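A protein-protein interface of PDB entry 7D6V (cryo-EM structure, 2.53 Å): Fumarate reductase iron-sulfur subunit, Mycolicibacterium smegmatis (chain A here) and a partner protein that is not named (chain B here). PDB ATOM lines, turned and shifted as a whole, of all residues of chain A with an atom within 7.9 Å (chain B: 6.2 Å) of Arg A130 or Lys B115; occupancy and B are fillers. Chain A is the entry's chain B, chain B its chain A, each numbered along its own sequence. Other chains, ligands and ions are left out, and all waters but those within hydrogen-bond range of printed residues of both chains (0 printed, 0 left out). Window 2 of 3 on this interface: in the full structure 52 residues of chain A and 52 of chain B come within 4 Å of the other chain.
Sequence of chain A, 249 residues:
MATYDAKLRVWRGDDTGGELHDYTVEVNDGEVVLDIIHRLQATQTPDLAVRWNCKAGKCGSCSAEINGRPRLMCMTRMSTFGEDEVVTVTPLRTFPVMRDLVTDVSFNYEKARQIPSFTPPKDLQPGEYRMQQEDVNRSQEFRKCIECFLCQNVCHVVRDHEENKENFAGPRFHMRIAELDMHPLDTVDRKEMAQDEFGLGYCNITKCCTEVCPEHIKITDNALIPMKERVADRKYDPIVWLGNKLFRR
O of Pro A126 touches OE2 of Glu B102, 3.8 Å away. Tyr A129 touches Glu B102 (CE2 to O, 3.5 Å). Tyr A129 touches Gly B114. O of Asp B113 touches CD of Arg A130, 3.7 Å away. NH2 of Arg A130 touches CE of Lys B115, at 3.7 Å. Glu B102 touches Met A131. Gln A132 touches Arg B110 (C to CG, 3.9 Å). Gln A132 touches Asp B113. Gly B114 touches Gln A132. CA of Asp B109 touches OE1 of Gln A133 (3.6 Å).
Leu A124 touches none of the printed residues of chain B. Of chain B, only Asp B113, Gly B114 and Lys B115 come within 4 Å of Arg A130. Printed residues of chain A within 4 Å of Glu B102: Pro A126 (3.8 Å), Tyr A129 (3.5 Å) and Met A131 (3.8 Å). Printed residues of chain A within 4 Å of Asp B113: Arg A130 and Gln A132. Gly B114 touches just these residues of chain A: Tyr A129 (3.8 Å), Arg A130 (3.3 Å), Met A131 (3.1 Å) and Gln A132 (3.8 Å). Lys B115 touches one residue of chain A. The nearest residue of chain B that does not touch Arg A130 is Arg B110 (4.3 Å). The nearest residue of chain A that does not touch Lys B115 is Met A131 (4.6 Å). The nearest printed residue of chain A that does not touch Lys B112 is Gln A133 (6.0 Å).
The backbone carbonyl oxygen (O) of Lys B112 sits close to the side-chain amide oxygen (OE1) of Gln A132 (3.5 Å). N of Met A131 sits at hydrogen-bond distance from O of Gly B114 (3.1 Å). NE of Arg B110 is in hydrogen-bond range of O of Met A131 (3.0 Å). N of Arg B110 lies within hydrogen-bond range of OE1 of Gln A133, at 3.0 Å.
Of the 14 printed residues of chain A, 6 touch a printed residue of chain B. Among the printed residues, 16 pairs touch across the chains. Among the printed residues, no Asp or Glu carboxylate lies within 4 Å of a Lys or Arg side-chain nitrogen of the other chain.
The backbone NH (N) of Lys B115 is in hydrogen-bond range of the side-chain hydroxyl (OG1) of Thr B111. The guanidinium group (NE) of Arg B110 lies close to the backbone carbonyl oxygen (O) of Lys B115 (3.5 Å). The backbone carbonyl oxygen (O) of Gly B114 lies within hydrogen-bond range of the guanidinium group (NH2) of Arg B110 (2.7 Å). The side-chain hydroxyl (OG1) of Thr B111 lies close to the backbone NH (N) of Asp B113, at 3.4 Å. OE1 of Glu B102 is in salt-bridge range of NH1 of Arg B110. The backbone carbonyl oxygen (O) of Asp B109 lies within hydrogen-bond range of the backbone NH (N) of Ser B117.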
ATOM      1  N   LEU A 124      13.173 -20.160  -3.101  1.00  0.00           N
ATOM      2  CA  LEU A 124      12.045 -19.907  -3.982  1.00  0.00           C
ATOM      3  C   LEU A 124      11.025 -21.035  -3.881  1.00  0.00           C
ATOM      4  O   LEU A 124      11.381 -22.215  -3.939  1.00  0.00           O
ATOM      5  CB  LEU A 124      12.543 -19.756  -5.420  1.00  0.00           C
ATOM      6  CG  LEU A 124      11.680 -19.013  -6.435  1.00  0.00           C
ATOM      7  CD1 LEU A 124      11.342 -17.629  -5.927  1.00  0.00           C
ATOM      8  CD2 LEU A 124      12.411 -18.926  -7.760  1.00  0.00           C
ATOM      9  N   GLN A 125       9.759 -20.667  -3.728  1.00  0.00           N
ATOM     10  CA  GLN A 125       8.658 -21.610  -3.632  1.00  0.00           C
ATOM     11  C   GLN A 125       8.160 -21.993  -5.017  1.00  0.00           C
ATOM     12  O   GLN A 125       8.353 -21.252  -5.984  1.00  0.00           O
ATOM     13  CB  GLN A 125       7.525 -21.005  -2.807  1.00  0.00           C
ATOM     14  CG  GLN A 125       7.963 -20.442  -1.462  1.00  0.00           C
ATOM     15  CD  GLN A 125       8.233 -21.515  -0.417  1.00  0.00           C
ATOM     16  OE1 GLN A 125       8.609 -22.641  -0.738  1.00  0.00           O
ATOM     17  NE2 GLN A 125       8.043 -21.160   0.848  1.00  0.00           N
ATOM     18  N   PRO A 126       7.522 -23.162  -5.148  1.00  0.00           N
ATOM     19  CA  PRO A 126       7.121 -23.628  -6.489  1.00  0.00           C
ATOM     20  C   PRO A 126       6.215 -22.671  -7.246  1.00  0.00           C
ATOM     21  O   PRO A 126       6.354 -22.539  -8.468  1.00  0.00           O
ATOM     22  CB  PRO A 126       6.418 -24.965  -6.199  1.00  0.00           C
ATOM     23  CG  PRO A 126       6.267 -25.037  -4.711  1.00  0.00           C
ATOM     24  CD  PRO A 126       7.357 -24.217  -4.138  1.00  0.00           C
ATOM     25  N   GLY A 127       5.295 -21.998  -6.567  1.00  0.00           N
ATOM     26  CA  GLY A 127       4.430 -21.059  -7.245  1.00  0.00           C
ATOM     27  C   GLY A 127       4.992 -19.669  -7.428  1.00  0.00           C
ATOM     28  O   GLY A 127       4.315 -18.808  -7.997  1.00  0.00           O
ATOM     29  N   GLU A 128       6.220 -19.418  -6.972  1.00  0.00           N
ATOM     30  CA  GLU A 128       6.787 -18.077  -6.945  1.00  0.00           C
ATOM     31  C   GLU A 128       7.879 -17.867  -7.985  1.00  0.00           C
ATOM     32  O   GLU A 128       8.574 -16.849  -7.938  1.00  0.00           O
ATOM     33  CB  GLU A 128       7.323 -17.766  -5.547  1.00  0.00           C
ATOM     34  N   TYR A 129       8.049 -18.797  -8.920  1.00  0.00           N
ATOM     35  CA  TYR A 129       9.028 -18.616  -9.982  1.00  0.00           C
ATOM     36  C   TYR A 129       8.569 -17.529 -10.947  1.00  0.00           C
ATOM     37  O   TYR A 129       7.389 -17.445 -11.294  1.00  0.00           O
ATOM     38  CB  TYR A 129       9.244 -19.925 -10.741  1.00  0.00           C
ATOM     39  CG  TYR A 129      10.103 -20.947 -10.029  1.00  0.00           C
ATOM     40  CD1 TYR A 129       9.919 -21.234  -8.685  1.00  0.00           C
ATOM     41  CD2 TYR A 129      11.094 -21.637 -10.712  1.00  0.00           C
ATOM     42  CE1 TYR A 129      10.700 -22.166  -8.042  1.00  0.00           C
ATOM     43  CE2 TYR A 129      11.881 -22.572 -10.076  1.00  0.00           C
ATOM     44  CZ  TYR A 129      11.679 -22.832  -8.741  1.00  0.00           C
ATOM     45  OH  TYR A 129      12.461 -23.764  -8.104  1.00  0.00           O
ATOM     46  N   ARG A 130       9.510 -16.694 -11.383  1.00  0.00           N
ATOM     47  CA  ARG A 130       9.226 -15.641 -12.352  1.00  0.00           C
ATOM     48  C   ARG A 130      10.330 -15.627 -13.396  1.00  0.00           C
ATOM     49  O   ARG A 130      11.499 -15.426 -13.058  1.00  0.00           O
ATOM     50  CB  ARG A 130       9.118 -14.269 -11.682  1.00  0.00           C
ATOM     51  CG  ARG A 130       7.989 -14.140 -10.688  1.00  0.00           C
ATOM     52  CD  ARG A 130       6.634 -14.148 -11.366  1.00  0.00           C
ATOM     53  NE  ARG A 130       5.561 -14.185 -10.380  1.00  0.00           N
ATOM     54  CZ  ARG A 130       4.919 -15.286 -10.012  1.00  0.00           C
ATOM     55  NH1 ARG A 130       5.235 -16.452 -10.554  1.00  0.00           N
ATOM     56  NH2 ARG A 130       3.962 -15.224  -9.101  1.00  0.00           N
ATOM     57  N   MET A 131       9.961 -15.834 -14.656  1.00  0.00           N
ATOM     58  CA  MET A 131      10.903 -15.776 -15.762  1.00  0.00           C
ATOM     59  C   MET A 131      10.255 -15.065 -16.937  1.00  0.00           C
ATOM     60  O   MET A 131       9.086 -15.303 -17.246  1.00  0.00           O
ATOM     61  CB  MET A 131      11.357 -17.177 -16.190  1.00  0.00           C
ATOM     62  CG  MET A 131      12.025 -17.984 -15.092  1.00  0.00           C
ATOM     63  SD  MET A 131      12.492 -19.637 -15.621  1.00  0.00           S
ATOM     64  CE  MET A 131      10.980 -20.528 -15.291  1.00  0.00           C
ATOM     65  N   GLN A 132      11.014 -14.194 -17.587  1.00  0.00           N
ATOM     66  CA  GLN A 132      10.563 -13.546 -18.808  1.00  0.00           C
ATOM     67  C   GLN A 132      10.880 -14.423 -20.016  1.00  0.00           C
ATOM     68  O   GLN A 132      11.786 -15.257 -19.987  1.00  0.00           O
ATOM     69  CB  GLN A 132      11.209 -12.170 -18.957  1.00  0.00           C
ATOM     70  CG  GLN A 132      10.912 -11.219 -17.807  1.00  0.00           C
ATOM     71  CD  GLN A 132       9.451 -10.816 -17.740  1.00  0.00           C
ATOM     72  OE1 GLN A 132       8.798 -10.638 -18.764  1.00  0.00           O
ATOM     73  NE2 GLN A 132       8.933 -10.670 -16.528  1.00  0.00           N
ATOM     74  N   GLN A 133      10.107 -14.226 -21.086  1.00  0.00           N
ATOM     75  CA  GLN A 133      10.232 -15.079 -22.265  1.00  0.00           C
ATOM     76  C   GLN A 133      11.603 -14.943 -22.920  1.00  0.00           C
ATOM     77  O   GLN A 133      12.209 -15.944 -23.331  1.00  0.00           O
ATOM     78  CB  GLN A 133       9.126 -14.748 -23.265  1.00  0.00           C
ATOM     79  CG  GLN A 133       9.125 -15.620 -24.501  1.00  0.00           C
ATOM     80  CD  GLN A 133       8.750 -17.053 -24.201  1.00  0.00           C
ATOM     81  OE1 GLN A 133       7.793 -17.316 -23.480  1.00  0.00           O
ATOM     82  NE2 GLN A 133       9.503 -17.990 -24.758  1.00  0.00           N
ATOM     83  N   ASP A 135      14.306 -14.315 -21.527  1.00  0.00           N
ATOM     84  CA  ASP A 135      15.283 -14.975 -20.676  1.00  0.00           C
ATOM     85  C   ASP A 135      15.278 -16.488 -20.839  1.00  0.00           C
ATOM     86  O   ASP A 135      16.238 -17.143 -20.423  1.00  0.00           O
ATOM     87  CB  ASP A 135      15.026 -14.627 -19.210  1.00  0.00           C
ATOM     88  CG  ASP A 135      15.410 -13.206 -18.873  1.00  0.00           C
ATOM     89  OD1 ASP A 135      15.813 -12.464 -19.787  1.00  0.00           O
ATOM     90  OD2 ASP A 135      15.308 -12.831 -17.686  1.00  0.00           O
ATOM     91  N   VAL A 136      14.230 -17.057 -21.430  1.00  0.00           N
ATOM     92  CA  VAL A 136      14.102 -18.505 -21.547  1.00  0.00           C
ATOM     93  C   VAL A 136      14.143 -18.998 -22.983  1.00  0.00           C
ATOM     94  O   VAL A 136      14.136 -20.220 -23.193  1.00  0.00           O
ATOM     95  CB  VAL A 136      12.819 -19.018 -20.859  1.00  0.00           C
ATOM     96  CG1 VAL A 136      12.703 -18.447 -19.459  1.00  0.00           C
ATOM     97  CG2 VAL A 136      11.594 -18.672 -21.687  1.00  0.00           C
ATOM     98  N   PRO A 184      17.768 -18.984 -16.646  1.00  0.00           N
ATOM     99  CA  PRO A 184      17.837 -17.763 -15.827  1.00  0.00           C
ATOM    100  C   PRO A 184      17.822 -18.008 -14.328  1.00  0.00           C
ATOM    101  O   PRO A 184      18.255 -17.131 -13.575  1.00  0.00           O
ATOM    102  CB  PRO A 184      16.603 -16.969 -16.276  1.00  0.00           C
ATOM    103  CG  PRO A 184      15.714 -17.963 -16.935  1.00  0.00           C
ATOM    104  CD  PRO A 184      16.603 -18.985 -17.545  1.00  0.00           C
ATOM    105  N   LEU A 185      17.342 -19.159 -13.866  1.00  0.00           N
ATOM    106  CA  LEU A 185      17.211 -19.416 -12.440  1.00  0.00           C
ATOM    107  C   LEU A 185      18.177 -20.469 -11.915  1.00  0.00           C
ATOM    108  O   LEU A 185      18.135 -20.780 -10.722  1.00  0.00           O
ATOM    109  CB  LEU A 185      15.771 -19.827 -12.111  1.00  0.00           C
ATOM    110  CG  LEU A 185      14.726 -18.716 -12.223  1.00  0.00           C
ATOM    111  CD1 LEU A 185      13.364 -19.221 -11.808  1.00  0.00           C
ATOM    112  CD2 LEU A 185      15.126 -17.518 -11.386  1.00  0.00           C
ATOM    113  N   ARG B  59      -4.800 -19.575 -12.832  1.00  0.00           N
ATOM    114  CA  ARG B  59      -5.343 -18.216 -12.873  1.00  0.00           C
ATOM    115  C   ARG B  59      -4.318 -17.192 -13.350  1.00  0.00           C
ATOM    116  O   ARG B  59      -4.411 -16.012 -13.012  1.00  0.00           O
ATOM    117  CB  ARG B  59      -5.914 -17.794 -11.515  1.00  0.00           C
ATOM    118  CG  ARG B  59      -7.016 -18.693 -11.000  1.00  0.00           C
ATOM    119  CD  ARG B  59      -7.135 -18.613  -9.493  1.00  0.00           C
ATOM    120  NE  ARG B  59      -7.837 -17.410  -9.060  1.00  0.00           N
ATOM    121  CZ  ARG B  59      -7.409 -16.600  -8.098  1.00  0.00           C
ATOM    122  NH1 ARG B  59      -6.276 -16.861  -7.466  1.00  0.00           N
ATOM    123  NH2 ARG B  59      -8.113 -15.528  -7.768  1.00  0.00           N
ATOM    124  N   ASN B  60      -3.341 -17.627 -14.146  1.00  0.00           N
ATOM    125  CA  ASN B  60      -2.298 -16.715 -14.602  1.00  0.00           C
ATOM    126  C   ASN B  60      -2.827 -15.735 -15.640  1.00  0.00           C
ATOM    127  O   ASN B  60      -2.453 -14.557 -15.635  1.00  0.00           O
ATOM    128  CB  ASN B  60      -1.120 -17.502 -15.171  1.00  0.00           C
ATOM    129  CG  ASN B  60      -0.398 -18.302 -14.120  1.00  0.00           C
ATOM    130  OD1 ASN B  60      -0.517 -18.033 -12.927  1.00  0.00           O
ATOM    131  ND2 ASN B  60       0.359 -19.297 -14.555  1.00  0.00           N
ATOM    132  N   GLU B 102       8.147 -27.006 -12.744  1.00  0.00           N
ATOM    133  CA  GLU B 102       9.197 -26.064 -13.107  1.00  0.00           C
ATOM    134  C   GLU B 102      10.229 -25.867 -12.007  1.00  0.00           C
ATOM    135  O   GLU B 102      11.262 -25.239 -12.259  1.00  0.00           O
ATOM    136  CB  GLU B 102       8.595 -24.718 -13.512  1.00  0.00           C
ATOM    137  CG  GLU B 102       7.821 -24.005 -12.437  1.00  0.00           C
ATOM    138  CD  GLU B 102       7.349 -22.643 -12.890  1.00  0.00           C
ATOM    139  OE1 GLU B 102       7.818 -22.181 -13.947  1.00  0.00           O
ATOM    140  OE2 GLU B 102       6.513 -22.033 -12.191  1.00  0.00           O
ATOM    141  N   ASP B 109       6.151 -21.558 -21.738  1.00  0.00           N
ATOM    142  CA  ASP B 109       6.022 -20.204 -22.250  1.00  0.00           C
ATOM    143  C   ASP B 109       5.588 -19.271 -21.127  1.00  0.00           C
ATOM    144  O   ASP B 109       4.933 -19.683 -20.168  1.00  0.00           O
ATOM    145  CB  ASP B 109       5.020 -20.156 -23.401  1.00  0.00           C
ATOM    146  CG  ASP B 109       5.562 -20.775 -24.669  1.00  0.00           C
ATOM    147  OD1 ASP B 109       4.755 -21.256 -25.488  1.00  0.00           O
ATOM    148  OD2 ASP B 109       6.795 -20.783 -24.850  1.00  0.00           O
ATOM    149  N   ARG B 110       5.965 -18.004 -21.246  1.00  0.00           N
ATOM    150  CA  ARG B 110       5.780 -17.046 -20.169  1.00  0.00           C
ATOM    151  C   ARG B 110       4.790 -15.962 -20.566  1.00  0.00           C
ATOM    152  O   ARG B 110       4.587 -15.680 -21.749  1.00  0.00           O
ATOM    153  CB  ARG B 110       7.111 -16.401 -19.768  1.00  0.00           C
ATOM    154  CG  ARG B 110       8.294 -17.348 -19.749  1.00  0.00           C
ATOM    155  CD  ARG B 110       8.085 -18.499 -18.780  1.00  0.00           C
ATOM    156  NE  ARG B 110       7.909 -18.051 -17.404  1.00  0.00           N
ATOM    157  CZ  ARG B 110       7.624 -18.860 -16.392  1.00  0.00           C
ATOM    158  NH1 ARG B 110       7.482 -20.157 -16.606  1.00  0.00           N
ATOM    159  NH2 ARG B 110       7.480 -18.377 -15.169  1.00  0.00           N
ATOM    160  N   THR B 111       4.165 -15.363 -19.555  1.00  0.00           N
ATOM    161  CA  THR B 111       3.329 -14.191 -19.736  1.00  0.00           C
ATOM    162  C   THR B 111       4.162 -12.925 -19.535  1.00  0.00           C
ATOM    163  O   THR B 111       5.373 -12.975 -19.310  1.00  0.00           O
ATOM    164  CB  THR B 111       2.140 -14.221 -18.776  1.00  0.00           C
ATOM    165  OG1 THR B 111       2.600 -14.023 -17.434  1.00  0.00           O
ATOM    166  CG2 THR B 111       1.419 -15.542 -18.863  1.00  0.00           C
ATOM    167  N   LYS B 112       3.501 -11.769 -19.625  1.00  0.00           N
ATOM    168  CA  LYS B 112       4.194 -10.503 -19.411  1.00  0.00           C
ATOM    169  C   LYS B 112       4.635 -10.336 -17.962  1.00  0.00           C
ATOM    170  O   LYS B 112       5.649  -9.683 -17.700  1.00  0.00           O
ATOM    171  CB  LYS B 112       3.297  -9.338 -19.828  1.00  0.00           C
ATOM    172  CG  LYS B 112       2.863  -9.322 -21.295  1.00  0.00           C
ATOM    173  CD  LYS B 112       3.999  -8.992 -22.259  1.00  0.00           C
ATOM    174  CE  LYS B 112       4.687 -10.230 -22.813  1.00  0.00           C
ATOM    175  NZ  LYS B 112       5.716  -9.878 -23.828  1.00  0.00           N
ATOM    176  N   ASP B 113       3.893 -10.908 -17.015  1.00  0.00           N
ATOM    177  CA  ASP B 113       4.269 -10.844 -15.609  1.00  0.00           C
ATOM    178  C   ASP B 113       5.354 -11.842 -15.239  1.00  0.00           C
ATOM    179  O   ASP B 113       5.843 -11.806 -14.106  1.00  0.00           O
ATOM    180  CB  ASP B 113       3.053 -11.094 -14.717  1.00  0.00           C
ATOM    181  CG  ASP B 113       1.852 -10.275 -15.123  1.00  0.00           C
ATOM    182  OD1 ASP B 113       2.022  -9.076 -15.424  1.00  0.00           O
ATOM    183  OD2 ASP B 113       0.737 -10.834 -15.136  1.00  0.00           O
ATOM    184  N   GLY B 114       5.732 -12.730 -16.151  1.00  0.00           N
ATOM    185  CA  GLY B 114       6.703 -13.756 -15.845  1.00  0.00           C
ATOM    186  C   GLY B 114       6.126 -15.036 -15.295  1.00  0.00           C
ATOM    187  O   GLY B 114       6.864 -15.816 -14.685  1.00  0.00           O
ATOM    188  N   LYS B 115       4.834 -15.276 -15.481  1.00  0.00           N
ATOM    189  CA  LYS B 115       4.186 -16.496 -15.034  1.00  0.00           C
ATOM    190  C   LYS B 115       4.078 -17.477 -16.196  1.00  0.00           C
ATOM    191  O   LYS B 115       4.522 -17.213 -17.312  1.00  0.00           O
ATOM    192  CB  LYS B 115       2.810 -16.187 -14.445  1.00  0.00           C
ATOM    193  CG  LYS B 115       2.812 -15.087 -13.412  1.00  0.00           C
ATOM    194  CD  LYS B 115       1.508 -15.059 -12.647  1.00  0.00           C
ATOM    195  CE  LYS B 115       1.524 -13.978 -11.587  1.00  0.00           C
ATOM    196  NZ  LYS B 115       0.569 -14.261 -10.485  1.00  0.00           N
ATOM    197  N   ILE B 116       3.477 -18.628 -15.925  1.00  0.00           N
ATOM    198  CA  ILE B 116       3.289 -19.649 -16.948  1.00  0.00           C
ATOM    199  C   ILE B 116       2.127 -19.246 -17.847  1.00  0.00           C
ATOM    200  O   ILE B 116       1.053 -18.871 -17.365  1.00  0.00           O
ATOM    201  CB  ILE B 116       3.051 -21.025 -16.307  1.00  0.00           C
ATOM    202  CG1 ILE B 116       4.287 -21.469 -15.526  1.00  0.00           C
ATOM    203  CG2 ILE B 116       2.718 -22.051 -17.363  1.00  0.00           C
ATOM    204  CD1 ILE B 116       4.146 -22.824 -14.885  1.00  0.00           C
ATOM    205  N   SER B 117       2.344 -19.313 -19.157  1.00  0.00           N
ATOM    206  CA  SER B 117       1.322 -18.946 -20.124  1.00  0.00           C
ATOM    207  C   SER B 117       0.284 -20.053 -20.258  1.00  0.00           C
ATOM    208  O   SER B 117       0.612 -21.241 -20.221  1.00  0.00           O
ATOM    209  CB  SER B 117       1.962 -18.657 -21.481  1.00  0.00           C
ATOM    210  OG  SER B 117       1.028 -18.087 -22.377  1.00  0.00           O
